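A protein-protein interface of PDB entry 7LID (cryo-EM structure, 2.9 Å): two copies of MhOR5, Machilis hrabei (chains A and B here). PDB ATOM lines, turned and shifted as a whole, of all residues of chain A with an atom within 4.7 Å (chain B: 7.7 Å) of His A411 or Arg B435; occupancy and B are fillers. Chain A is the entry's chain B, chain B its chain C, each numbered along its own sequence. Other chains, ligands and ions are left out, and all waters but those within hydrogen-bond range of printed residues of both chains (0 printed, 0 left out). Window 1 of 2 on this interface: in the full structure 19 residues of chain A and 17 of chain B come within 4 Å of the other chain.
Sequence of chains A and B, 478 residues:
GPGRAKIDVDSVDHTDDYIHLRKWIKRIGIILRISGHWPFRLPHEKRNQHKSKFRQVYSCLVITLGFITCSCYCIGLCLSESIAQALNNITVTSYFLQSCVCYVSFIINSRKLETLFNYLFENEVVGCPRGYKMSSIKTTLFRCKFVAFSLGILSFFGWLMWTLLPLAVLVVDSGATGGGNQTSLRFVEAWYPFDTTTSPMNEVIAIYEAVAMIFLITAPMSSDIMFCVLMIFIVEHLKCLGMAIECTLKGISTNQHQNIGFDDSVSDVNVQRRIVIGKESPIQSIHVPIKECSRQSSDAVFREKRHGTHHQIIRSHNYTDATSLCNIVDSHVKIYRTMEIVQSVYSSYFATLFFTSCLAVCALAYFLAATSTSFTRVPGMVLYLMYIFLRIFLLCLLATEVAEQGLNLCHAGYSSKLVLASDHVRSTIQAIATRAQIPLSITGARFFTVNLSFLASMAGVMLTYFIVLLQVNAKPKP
A ring nitrogen (ND1) of His B332 sits at hydrogen-bond distance from the side-chain hydroxyl (OH) of Tyr A414, at 3.2 Å. The side-chain hydroxyl (OG1) of Thr B434 lies within hydrogen-bond range of the side-chain amide nitrogen (NE2) of Gln A430, at 3.0 Å.
OH of Tyr B336 is in hydrogen-bond range of OE1 of Glu B340. The side-chain hydroxyl (OG1) of Thr B434 is in hydrogen-bond range of the backbone carbonyl oxygen (O) of Gln B430 (3.0 Å).
Among the printed residues, pairs that only touch across the chains: Leu A407 with Ile B438 (3.9 Å), Asn A408 with Tyr B336 (3.7 Å), Cys A410 with Arg B435 (3.7 Å), Cys A410 with Ile B438 (3.8 Å), His A411 with Tyr B336 (3.7 Å), His A411 with Arg B435 (3.7 Å), His A411 with Ile B438 (3.8 Å), Ala A412 with Arg B435 (3.9 Å), Tyr A414 with Val B333 (3.1 Å), Tyr A414 with Ile B432 (3.6 Å), Tyr A414 with Arg B435 (3.7 Å), Ile A429 with Arg B435 (3.3 Å), Gln A430 with Ala B431 (3.8 Å), Gln A430 with Arg B435 (3.8 Å) and Ala A433 with Arg B435 (3.5 Å).
Of the printed residues of chain B, Leu A407 touches Ile B438 (3.9 Å). Of the printed residues of chain A, Tyr B336 touches Asn A408 (3.7 Å) and His A411 (3.7 Å). Printed residues of chain A within 4 Å of Thr B434: Gln A430 (3.0 Å). Cys B410 touches none of the printed residues of chain A. Arg B337 touches none of the printed residues of chain A. The nearest residue of chain A that does not touch Arg B435 is Leu A418 (4.5 Å). The nearest printed residue of chain B that does not touch Asn A408 is Glu B340 (4.7 Å).
Printed residues of chain B that touch a printed residue of chain A: His B332, Val B333, Tyr B336, Ala B431, Ile B432, Thr B434, Arg B435 and Ile B438. Among the printed residues, 17 pairs touch across the chains. Among the printed residues, no Asp or Glu carboxylate lies within 4 Å of a Lys or Arg side-chain nitrogen of the other chain.
5 positions are printed for both chains. Of the 17 pairs that touch across the chains among the printed residues, none has its exchanged pair printed and touching as well.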
ATOM      1  N   LEU A 407     -16.636   8.552  11.572  1.00  0.00           N
ATOM      2  CA  LEU A 407     -16.741  10.008  11.496  1.00  0.00           C
ATOM      3  C   LEU A 407     -17.933  10.438  10.644  1.00  0.00           C
ATOM      4  O   LEU A 407     -18.437  11.556  10.787  1.00  0.00           O
ATOM      5  CB  LEU A 407     -15.443  10.608  10.957  1.00  0.00           C
ATOM      6  CG  LEU A 407     -14.418  11.087  11.987  1.00  0.00           C
ATOM      7  CD1 LEU A 407     -15.029  12.155  12.862  1.00  0.00           C
ATOM      8  CD2 LEU A 407     -13.877   9.951  12.832  1.00  0.00           C
ATOM      9  N   ASN A 408     -18.398   9.565   9.746  1.00  0.00           N
ATOM     10  CA  ASN A 408     -19.639   9.854   9.034  1.00  0.00           C
ATOM     11  C   ASN A 408     -20.860   9.499   9.872  1.00  0.00           C
ATOM     12  O   ASN A 408     -21.955  10.010   9.619  1.00  0.00           O
ATOM     13  CB  ASN A 408     -19.669   9.108   7.703  1.00  0.00           C
ATOM     14  CG  ASN A 408     -18.788   9.754   6.660  1.00  0.00           C
ATOM     15  OD1 ASN A 408     -17.978  10.625   6.972  1.00  0.00           O
ATOM     16  ND2 ASN A 408     -18.940   9.332   5.412  1.00  0.00           N
ATOM     17  N   LEU A 409     -20.697   8.618  10.861  1.00  0.00           N
ATOM     18  CA  LEU A 409     -21.766   8.381  11.826  1.00  0.00           C
ATOM     19  C   LEU A 409     -21.905   9.558  12.781  1.00  0.00           C
ATOM     20  O   LEU A 409     -22.954   9.734  13.410  1.00  0.00           O
ATOM     21  CB  LEU A 409     -21.502   7.087  12.598  1.00  0.00           C
ATOM     22  CG  LEU A 409     -22.605   6.520  13.489  1.00  0.00           C
ATOM     23  CD1 LEU A 409     -23.769   6.067  12.647  1.00  0.00           C
ATOM     24  CD2 LEU A 409     -22.077   5.380  14.329  1.00  0.00           C
ATOM     25  N   CYS A 410     -20.847  10.365  12.912  1.00  0.00           N
ATOM     26  CA  CYS A 410     -20.969  11.617  13.662  1.00  0.00           C
ATOM     27  C   CYS A 410     -21.995  12.559  13.031  1.00  0.00           C
ATOM     28  O   CYS A 410     -22.744  13.235  13.745  1.00  0.00           O
ATOM     29  CB  CYS A 410     -19.612  12.310  13.764  1.00  0.00           C
ATOM     30  SG  CYS A 410     -19.576  13.702  14.909  1.00  0.00           S
ATOM     31  N   HIS A 411     -22.044  12.619  11.703  1.00  0.00           N
ATOM     32  CA  HIS A 411     -23.006  13.461  10.985  1.00  0.00           C
ATOM     33  C   HIS A 411     -24.282  12.701  10.641  1.00  0.00           C
ATOM     34  O   HIS A 411     -24.722  12.693   9.495  1.00  0.00           O
ATOM     35  CB  HIS A 411     -22.368  14.014   9.717  1.00  0.00           C
ATOM     36  CG  HIS A 411     -21.642  15.304   9.911  1.00  0.00           C
ATOM     37  ND1 HIS A 411     -22.292  16.510  10.053  1.00  0.00           N
ATOM     38  CD2 HIS A 411     -20.318  15.582   9.966  1.00  0.00           C
ATOM     39  CE1 HIS A 411     -21.401  17.474  10.199  1.00  0.00           C
ATOM     40  NE2 HIS A 411     -20.196  16.937  10.149  1.00  0.00           N
ATOM     41  N   ALA A 412     -24.901  12.065  11.628  1.00  0.00           N
ATOM     42  CA  ALA A 412     -26.086  11.259  11.391  1.00  0.00           C
ATOM     43  C   ALA A 412     -27.257  11.820  12.179  1.00  0.00           C
ATOM     44  O   ALA A 412     -27.130  12.136  13.364  1.00  0.00           O
ATOM     45  CB  ALA A 412     -25.859   9.798  11.773  1.00  0.00           C
ATOM     46  N   GLY A 413     -28.399  11.930  11.511  1.00  0.00           N
ATOM     47  CA  GLY A 413     -29.585  12.464  12.159  1.00  0.00           C
ATOM     48  C   GLY A 413     -29.478  13.936  12.480  1.00  0.00           C
ATOM     49  O   GLY A 413     -29.749  14.345  13.614  1.00  0.00           O
ATOM     50  N   TYR A 414     -29.080  14.743  11.506  1.00  0.00           N
ATOM     51  CA  TYR A 414     -28.827  16.166  11.706  1.00  0.00           C
ATOM     52  C   TYR A 414     -29.579  16.897  10.602  1.00  0.00           C
ATOM     53  O   TYR A 414     -29.099  16.975   9.470  1.00  0.00           O
ATOM     54  CB  TYR A 414     -27.328  16.444  11.679  1.00  0.00           C
ATOM     55  CG  TYR A 414     -26.909  17.879  11.874  1.00  0.00           C
ATOM     56  CD1 TYR A 414     -27.444  18.650  12.891  1.00  0.00           C
ATOM     57  CD2 TYR A 414     -25.937  18.446  11.065  1.00  0.00           C
ATOM     58  CE1 TYR A 414     -27.041  19.955  13.075  1.00  0.00           C
ATOM     59  CE2 TYR A 414     -25.531  19.746  11.242  1.00  0.00           C
ATOM     60  CZ  TYR A 414     -26.085  20.494  12.247  1.00  0.00           C
ATOM     61  OH  TYR A 414     -25.686  21.793  12.432  1.00  0.00           O
ATOM     62  N   LEU A 418     -34.164  17.367  13.931  1.00  0.00           N
ATOM     63  CA  LEU A 418     -33.452  17.443  15.206  1.00  0.00           C
ATOM     64  C   LEU A 418     -33.781  18.719  15.963  1.00  0.00           C
ATOM     65  O   LEU A 418     -33.897  18.698  17.193  1.00  0.00           O
ATOM     66  CB  LEU A 418     -31.945  17.358  14.969  1.00  0.00           C
ATOM     67  CG  LEU A 418     -31.060  17.308  16.212  1.00  0.00           C
ATOM     68  CD1 LEU A 418     -30.974  15.891  16.709  1.00  0.00           C
ATOM     69  CD2 LEU A 418     -29.682  17.861  15.922  1.00  0.00           C
ATOM     70  N   ILE A 429     -29.085  12.032  20.665  1.00  0.00           N
ATOM     71  CA  ILE A 429     -28.309  12.220  19.440  1.00  0.00           C
ATOM     72  C   ILE A 429     -27.009  12.958  19.748  1.00  0.00           C
ATOM     73  O   ILE A 429     -25.959  12.673  19.159  1.00  0.00           O
ATOM     74  CB  ILE A 429     -29.158  12.949  18.380  1.00  0.00           C
ATOM     75  CG1 ILE A 429     -30.367  12.103  17.995  1.00  0.00           C
ATOM     76  CG2 ILE A 429     -28.365  13.225  17.128  1.00  0.00           C
ATOM     77  CD1 ILE A 429     -30.013  10.755  17.459  1.00  0.00           C
ATOM     78  N   GLN A 430     -27.049  13.875  20.718  1.00  0.00           N
ATOM     79  CA  GLN A 430     -25.837  14.563  21.152  1.00  0.00           C
ATOM     80  C   GLN A 430     -24.855  13.600  21.812  1.00  0.00           C
ATOM     81  O   GLN A 430     -23.644  13.680  21.572  1.00  0.00           O
ATOM     82  CB  GLN A 430     -26.200  15.697  22.107  1.00  0.00           C
ATOM     83  CG  GLN A 430     -25.011  16.469  22.631  1.00  0.00           C
ATOM     84  CD  GLN A 430     -24.287  17.211  21.537  1.00  0.00           C
ATOM     85  OE1 GLN A 430     -24.908  17.730  20.612  1.00  0.00           O
ATOM     86  NE2 GLN A 430     -22.967  17.268  21.636  1.00  0.00           N
ATOM     87  N   ALA A 433     -23.301  11.499  19.051  1.00  0.00           N
ATOM     88  CA  ALA A 433     -22.298  12.246  18.296  1.00  0.00           C
ATOM     89  C   ALA A 433     -21.016  12.429  19.101  1.00  0.00           C
ATOM     90  O   ALA A 433     -19.908  12.337  18.555  1.00  0.00           O
ATOM     91  CB  ALA A 433     -22.862  13.599  17.873  1.00  0.00           C
ATOM     92  N   HIS B 332     -26.334  24.401   6.668  1.00  0.00           N
ATOM     93  CA  HIS B 332     -25.113  23.735   7.115  1.00  0.00           C
ATOM     94  C   HIS B 332     -25.031  22.310   6.580  1.00  0.00           C
ATOM     95  O   HIS B 332     -23.963  21.856   6.138  1.00  0.00           O
ATOM     96  CB  HIS B 332     -25.060  23.737   8.641  1.00  0.00           C
ATOM     97  CG  HIS B 332     -23.702  23.463   9.203  1.00  0.00           C
ATOM     98  ND1 HIS B 332     -23.492  23.194  10.536  1.00  0.00           N
ATOM     99  CD2 HIS B 332     -22.484  23.422   8.614  1.00  0.00           C
ATOM    100  CE1 HIS B 332     -22.204  22.995  10.746  1.00  0.00           C
ATOM    101  NE2 HIS B 332     -21.571  23.128   9.596  1.00  0.00           N
ATOM    102  N   VAL B 333     -26.163  21.605   6.575  1.00  0.00           N
ATOM    103  CA  VAL B 333     -26.192  20.237   6.068  1.00  0.00           C
ATOM    104  C   VAL B 333     -25.972  20.218   4.560  1.00  0.00           C
ATOM    105  O   VAL B 333     -25.276  19.338   4.035  1.00  0.00           O
ATOM    106  CB  VAL B 333     -27.512  19.563   6.491  1.00  0.00           C
ATOM    107  CG1 VAL B 333     -28.036  18.590   5.447  1.00  0.00           C
ATOM    108  CG2 VAL B 333     -27.293  18.852   7.787  1.00  0.00           C
ATOM    109  N   TYR B 336     -22.267  20.598   4.000  1.00  0.00           N
ATOM    110  CA  TYR B 336     -21.542  19.359   4.281  1.00  0.00           C
ATOM    111  C   TYR B 336     -21.751  18.319   3.181  1.00  0.00           C
ATOM    112  O   TYR B 336     -20.800  17.639   2.772  1.00  0.00           O
ATOM    113  CB  TYR B 336     -21.962  18.798   5.637  1.00  0.00           C
ATOM    114  CG  TYR B 336     -21.552  17.363   5.854  1.00  0.00           C
ATOM    115  CD1 TYR B 336     -20.212  17.008   5.943  1.00  0.00           C
ATOM    116  CD2 TYR B 336     -22.504  16.360   5.972  1.00  0.00           C
ATOM    117  CE1 TYR B 336     -19.833  15.693   6.142  1.00  0.00           C
ATOM    118  CE2 TYR B 336     -22.135  15.043   6.172  1.00  0.00           C
ATOM    119  CZ  TYR B 336     -20.800  14.716   6.256  1.00  0.00           C
ATOM    120  OH  TYR B 336     -20.436  13.407   6.454  1.00  0.00           O
ATOM    121  N   ARG B 337     -22.981  18.201   2.668  1.00  0.00           N
ATOM    122  CA  ARG B 337     -23.247  17.250   1.589  1.00  0.00           C
ATOM    123  C   ARG B 337     -22.552  17.666   0.297  1.00  0.00           C
ATOM    124  O   ARG B 337     -22.071  16.810  -0.456  1.00  0.00           O
ATOM    125  CB  ARG B 337     -24.750  17.112   1.353  1.00  0.00           C
ATOM    126  CG  ARG B 337     -25.515  16.509   2.509  1.00  0.00           C
ATOM    127  CD  ARG B 337     -25.510  14.995   2.480  1.00  0.00           C
ATOM    128  NE  ARG B 337     -25.719  14.436   3.812  1.00  0.00           N
ATOM    129  CZ  ARG B 337     -26.908  14.298   4.392  1.00  0.00           C
ATOM    130  NH1 ARG B 337     -28.011  14.673   3.757  1.00  0.00           N
ATOM    131  NH2 ARG B 337     -26.994  13.781   5.609  1.00  0.00           N
ATOM    132  N   GLU B 340     -19.003  16.703   0.622  1.00  0.00           N
ATOM    133  CA  GLU B 340     -18.888  15.255   0.461  1.00  0.00           C
ATOM    134  C   GLU B 340     -18.976  14.847  -1.008  1.00  0.00           C
ATOM    135  O   GLU B 340     -18.289  13.916  -1.442  1.00  0.00           O
ATOM    136  CB  GLU B 340     -19.967  14.553   1.284  1.00  0.00           C
ATOM    137  CG  GLU B 340     -19.965  13.042   1.175  1.00  0.00           C
ATOM    138  CD  GLU B 340     -21.032  12.395   2.031  1.00  0.00           C
ATOM    139  OE1 GLU B 340     -21.176  12.796   3.204  1.00  0.00           O
ATOM    140  OE2 GLU B 340     -21.725  11.485   1.532  1.00  0.00           O
ATOM    141  N   GLY B 406     -15.001  26.711   8.667  1.00  0.00           N
ATOM    142  CA  GLY B 406     -15.782  25.800   9.493  1.00  0.00           C
ATOM    143  C   GLY B 406     -15.441  25.918  10.967  1.00  0.00           C
ATOM    144  O   GLY B 406     -16.330  26.005  11.829  1.00  0.00           O
ATOM    145  N   LEU B 409     -16.942  28.836  12.220  1.00  0.00           N
ATOM    146  CA  LEU B 409     -18.372  28.639  12.442  1.00  0.00           C
ATOM    147  C   LEU B 409     -18.620  27.948  13.775  1.00  0.00           C
ATOM    148  O   LEU B 409     -19.726  28.023  14.323  1.00  0.00           O
ATOM    149  CB  LEU B 409     -18.978  27.831  11.294  1.00  0.00           C
ATOM    150  CG  LEU B 409     -20.497  27.708  11.198  1.00  0.00           C
ATOM    151  CD1 LEU B 409     -21.108  29.052  10.899  1.00  0.00           C
ATOM    152  CD2 LEU B 409     -20.882  26.697  10.144  1.00  0.00           C
ATOM    153  N   CYS B 410     -17.605  27.256  14.304  1.00  0.00           N
ATOM    154  CA  CYS B 410     -17.709  26.727  15.665  1.00  0.00           C
ATOM    155  C   CYS B 410     -17.887  27.841  16.697  1.00  0.00           C
ATOM    156  O   CYS B 410     -18.645  27.685  17.660  1.00  0.00           O
ATOM    157  CB  CYS B 410     -16.478  25.889  16.004  1.00  0.00           C
ATOM    158  SG  CYS B 410     -16.623  24.946  17.534  1.00  0.00           S
ATOM    159  N   SER B 427     -29.552  24.415  23.298  1.00  0.00           N
ATOM    160  CA  SER B 427     -29.276  23.073  22.806  1.00  0.00           C
ATOM    161  C   SER B 427     -28.997  23.042  21.310  1.00  0.00           C
ATOM    162  O   SER B 427     -28.139  22.274  20.861  1.00  0.00           O
ATOM    163  CB  SER B 427     -30.445  22.140  23.126  1.00  0.00           C
ATOM    164  OG  SER B 427     -30.365  21.675  24.460  1.00  0.00           O
ATOM    165  N   THR B 428     -29.679  23.883  20.528  1.00  0.00           N
ATOM    166  CA  THR B 428     -29.467  23.872  19.084  1.00  0.00           C
ATOM    167  C   THR B 428     -28.113  24.465  18.712  1.00  0.00           C
ATOM    168  O   THR B 428     -27.434  23.957  17.811  1.00  0.00           O
ATOM    169  CB  THR B 428     -30.593  24.625  18.386  1.00  0.00           C
ATOM    170  OG1 THR B 428     -31.835  24.313  19.023  1.00  0.00           O
ATOM    171  CG2 THR B 428     -30.672  24.211  16.941  1.00  0.00           C
ATOM    172  N   ILE B 429     -27.692  25.529  19.406  1.00  0.00           N
ATOM    173  CA  ILE B 429     -26.370  26.104  19.159  1.00  0.00           C
ATOM    174  C   ILE B 429     -25.281  25.129  19.595  1.00  0.00           C
ATOM    175  O   ILE B 429     -24.228  25.019  18.951  1.00  0.00           O
ATOM    176  CB  ILE B 429     -26.248  27.470  19.863  1.00  0.00           C
ATOM    177  CG1 ILE B 429     -27.259  28.456  19.289  1.00  0.00           C
ATOM    178  CG2 ILE B 429     -24.871  28.062  19.691  1.00  0.00           C
ATOM    179  CD1 ILE B 429     -27.117  28.677  17.816  1.00  0.00           C
ATOM    180  N   GLN B 430     -25.541  24.367  20.660  1.00  0.00           N
ATOM    181  CA  GLN B 430     -24.602  23.335  21.093  1.00  0.00           C
ATOM    182  C   GLN B 430     -24.480  22.221  20.058  1.00  0.00           C
ATOM    183  O   GLN B 430     -23.373  21.739  19.787  1.00  0.00           O
ATOM    184  CB  GLN B 430     -25.041  22.770  22.441  1.00  0.00           C
ATOM    185  CG  GLN B 430     -24.143  21.681  22.978  1.00  0.00           C
ATOM    186  CD  GLN B 430     -22.760  22.187  23.295  1.00  0.00           C
ATOM    187  OE1 GLN B 430     -22.594  23.309  23.768  1.00  0.00           O
ATOM    188  NE2 GLN B 430     -21.753  21.363  23.038  1.00  0.00           N
ATOM    189  N   ALA B 431     -25.604  21.815  19.460  1.00  0.00           N
ATOM    190  CA  ALA B 431     -25.568  20.801  18.409  1.00  0.00           C
ATOM    191  C   ALA B 431     -24.830  21.310  17.176  1.00  0.00           C
ATOM    192  O   ALA B 431     -24.060  20.569  16.549  1.00  0.00           O
ATOM    193  CB  ALA B 431     -26.988  20.371  18.045  1.00  0.00           C
ATOM    194  N   ILE B 432     -25.041  22.584  16.828  1.00  0.00           N
ATOM    195  CA  ILE B 432     -24.357  23.184  15.684  1.00  0.00           C
ATOM    196  C   ILE B 432     -22.854  23.252  15.928  1.00  0.00           C
ATOM    197  O   ILE B 432     -22.054  22.946  15.037  1.00  0.00           O
ATOM    198  CB  ILE B 432     -24.955  24.571  15.380  1.00  0.00           C
ATOM    199  CG1 ILE B 432     -26.340  24.422  14.757  1.00  0.00           C
ATOM    200  CG2 ILE B 432     -24.071  25.373  14.447  1.00  0.00           C
ATOM    201  CD1 ILE B 432     -27.050  25.729  14.553  1.00  0.00           C
ATOM    202  N   ALA B 433     -22.445  23.591  17.153  1.00  0.00           N
ATOM    203  CA  ALA B 433     -21.021  23.660  17.470  1.00  0.00           C
ATOM    204  C   ALA B 433     -20.382  22.275  17.477  1.00  0.00           C
ATOM    205  O   ALA B 433     -19.248  22.101  17.011  1.00  0.00           O
ATOM    206  CB  ALA B 433     -20.818  24.350  18.816  1.00  0.00           C
ATOM    207  N   THR B 434     -21.101  21.277  17.999  1.00  0.00           N
ATOM    208  CA  THR B 434     -20.580  19.912  18.026  1.00  0.00           C
ATOM    209  C   THR B 434     -20.409  19.361  16.613  1.00  0.00           C
ATOM    210  O   THR B 434     -19.403  18.714  16.304  1.00  0.00           O
ATOM    211  CB  THR B 434     -21.506  19.019  18.857  1.00  0.00           C
ATOM    212  OG1 THR B 434     -21.506  19.470  20.216  1.00  0.00           O
ATOM    213  CG2 THR B 434     -21.044  17.574  18.831  1.00  0.00           C
ATOM    214  N   ARG B 435     -21.366  19.646  15.726  1.00  0.00           N
ATOM    215  CA  ARG B 435     -21.221  19.200  14.343  1.00  0.00           C
ATOM    216  C   ARG B 435     -20.187  20.030  13.592  1.00  0.00           C
ATOM    217  O   ARG B 435     -19.581  19.550  12.628  1.00  0.00           O
ATOM    218  CB  ARG B 435     -22.564  19.257  13.622  1.00  0.00           C
ATOM    219  CG  ARG B 435     -23.280  17.934  13.571  1.00  0.00           C
ATOM    220  CD  ARG B 435     -23.988  17.665  14.874  1.00  0.00           C
ATOM    221  NE  ARG B 435     -24.472  16.296  14.951  1.00  0.00           N
ATOM    222  CZ  ARG B 435     -25.187  15.822  15.960  1.00  0.00           C
ATOM    223  NH1 ARG B 435     -25.499  16.609  16.977  1.00  0.00           N
ATOM    224  NH2 ARG B 435     -25.588  14.561  15.952  1.00  0.00           N
ATOM    225  N   ALA B 436     -19.973  21.278  14.010  1.00  0.00           N
ATOM    226  CA  ALA B 436     -19.034  22.138  13.301  1.00  0.00           C
ATOM    227  C   ALA B 436     -17.602  21.888  13.747  1.00  0.00           C
ATOM    228  O   ALA B 436     -16.658  22.344  13.094  1.00  0.00           O
ATOM    229  CB  ALA B 436     -19.408  23.603  13.504  1.00  0.00           C
ATOM    230  N   GLN B 437     -17.418  21.178  14.864  1.00  0.00           N
ATOM    231  CA  GLN B 437     -16.069  20.787  15.265  1.00  0.00           C
ATOM    232  C   GLN B 437     -15.456  19.776  14.303  1.00  0.00           C
ATOM    233  O   GLN B 437     -14.230  19.646  14.237  1.00  0.00           O
ATOM    234  CB  GLN B 437     -16.081  20.215  16.680  1.00  0.00           C
ATOM    235  CG  GLN B 437     -15.647  21.194  17.745  1.00  0.00           C
ATOM    236  CD  GLN B 437     -15.469  20.530  19.088  1.00  0.00           C
ATOM    237  OE1 GLN B 437     -15.390  19.307  19.179  1.00  0.00           O
ATOM    238  NE2 GLN B 437     -15.409  21.331  20.142  1.00  0.00           N
ATOM    239  N   ILE B 438     -16.288  19.045  13.565  1.00  0.00           N
ATOM    240  CA  ILE B 438     -15.773  18.150  12.523  1.00  0.00           C
ATOM    241  C   ILE B 438     -15.271  18.988  11.357  1.00  0.00           C
ATOM    242  O   ILE B 438     -16.023  19.840  10.841  1.00  0.00           O
ATOM    243  CB  ILE B 438     -16.867  17.171  12.067  1.00  0.00           C
ATOM    244  CG1 ILE B 438     -17.375  16.348  13.248  1.00  0.00           C
ATOM    245  CG2 ILE B 438     -16.350  16.264  10.973  1.00  0.00           C
ATOM    246  CD1 ILE B 438     -16.288  15.639  14.008  1.00  0.00           C
ATOM    247  N   PRO B 439     -14.034  18.810  10.897  1.00  0.00           N
ATOM    248  CA  PRO B 439     -13.510  19.678   9.836  1.00  0.00           C
ATOM    249  C   PRO B 439     -13.952  19.249   8.446  1.00  0.00           C
ATOM    250  O   PRO B 439     -14.050  18.063   8.127  1.00  0.00           O
ATOM    251  CB  PRO B 439     -11.992  19.525   9.998  1.00  0.00           C
ATOM    252  CG  PRO B 439     -11.819  18.154  10.528  1.00  0.00           C
ATOM    253  CD  PRO B 439     -13.019  17.864  11.389  1.00  0.00           C
ATOM    254  N   LEU B 440     -14.233  20.245   7.610  1.00  0.00           N
ATOM    255  CA  LEU B 440     -14.551  20.019   6.201  1.00  0.00           C
ATOM    256  C   LEU B 440     -13.240  20.052   5.430  1.00  0.00           C
ATOM    257  O   LEU B 440     -12.720  21.123   5.116  1.00  0.00           O
ATOM    258  CB  LEU B 440     -15.521  21.074   5.682  1.00  0.00           C
ATOM    259  CG  LEU B 440     -16.729  21.443   6.536  1.00  0.00           C
ATOM    260  CD1 LEU B 440     -17.545  22.502   5.836  1.00  0.00           C
ATOM    261  CD2 LEU B 440     -17.577  20.222   6.808  1.00  0.00           C
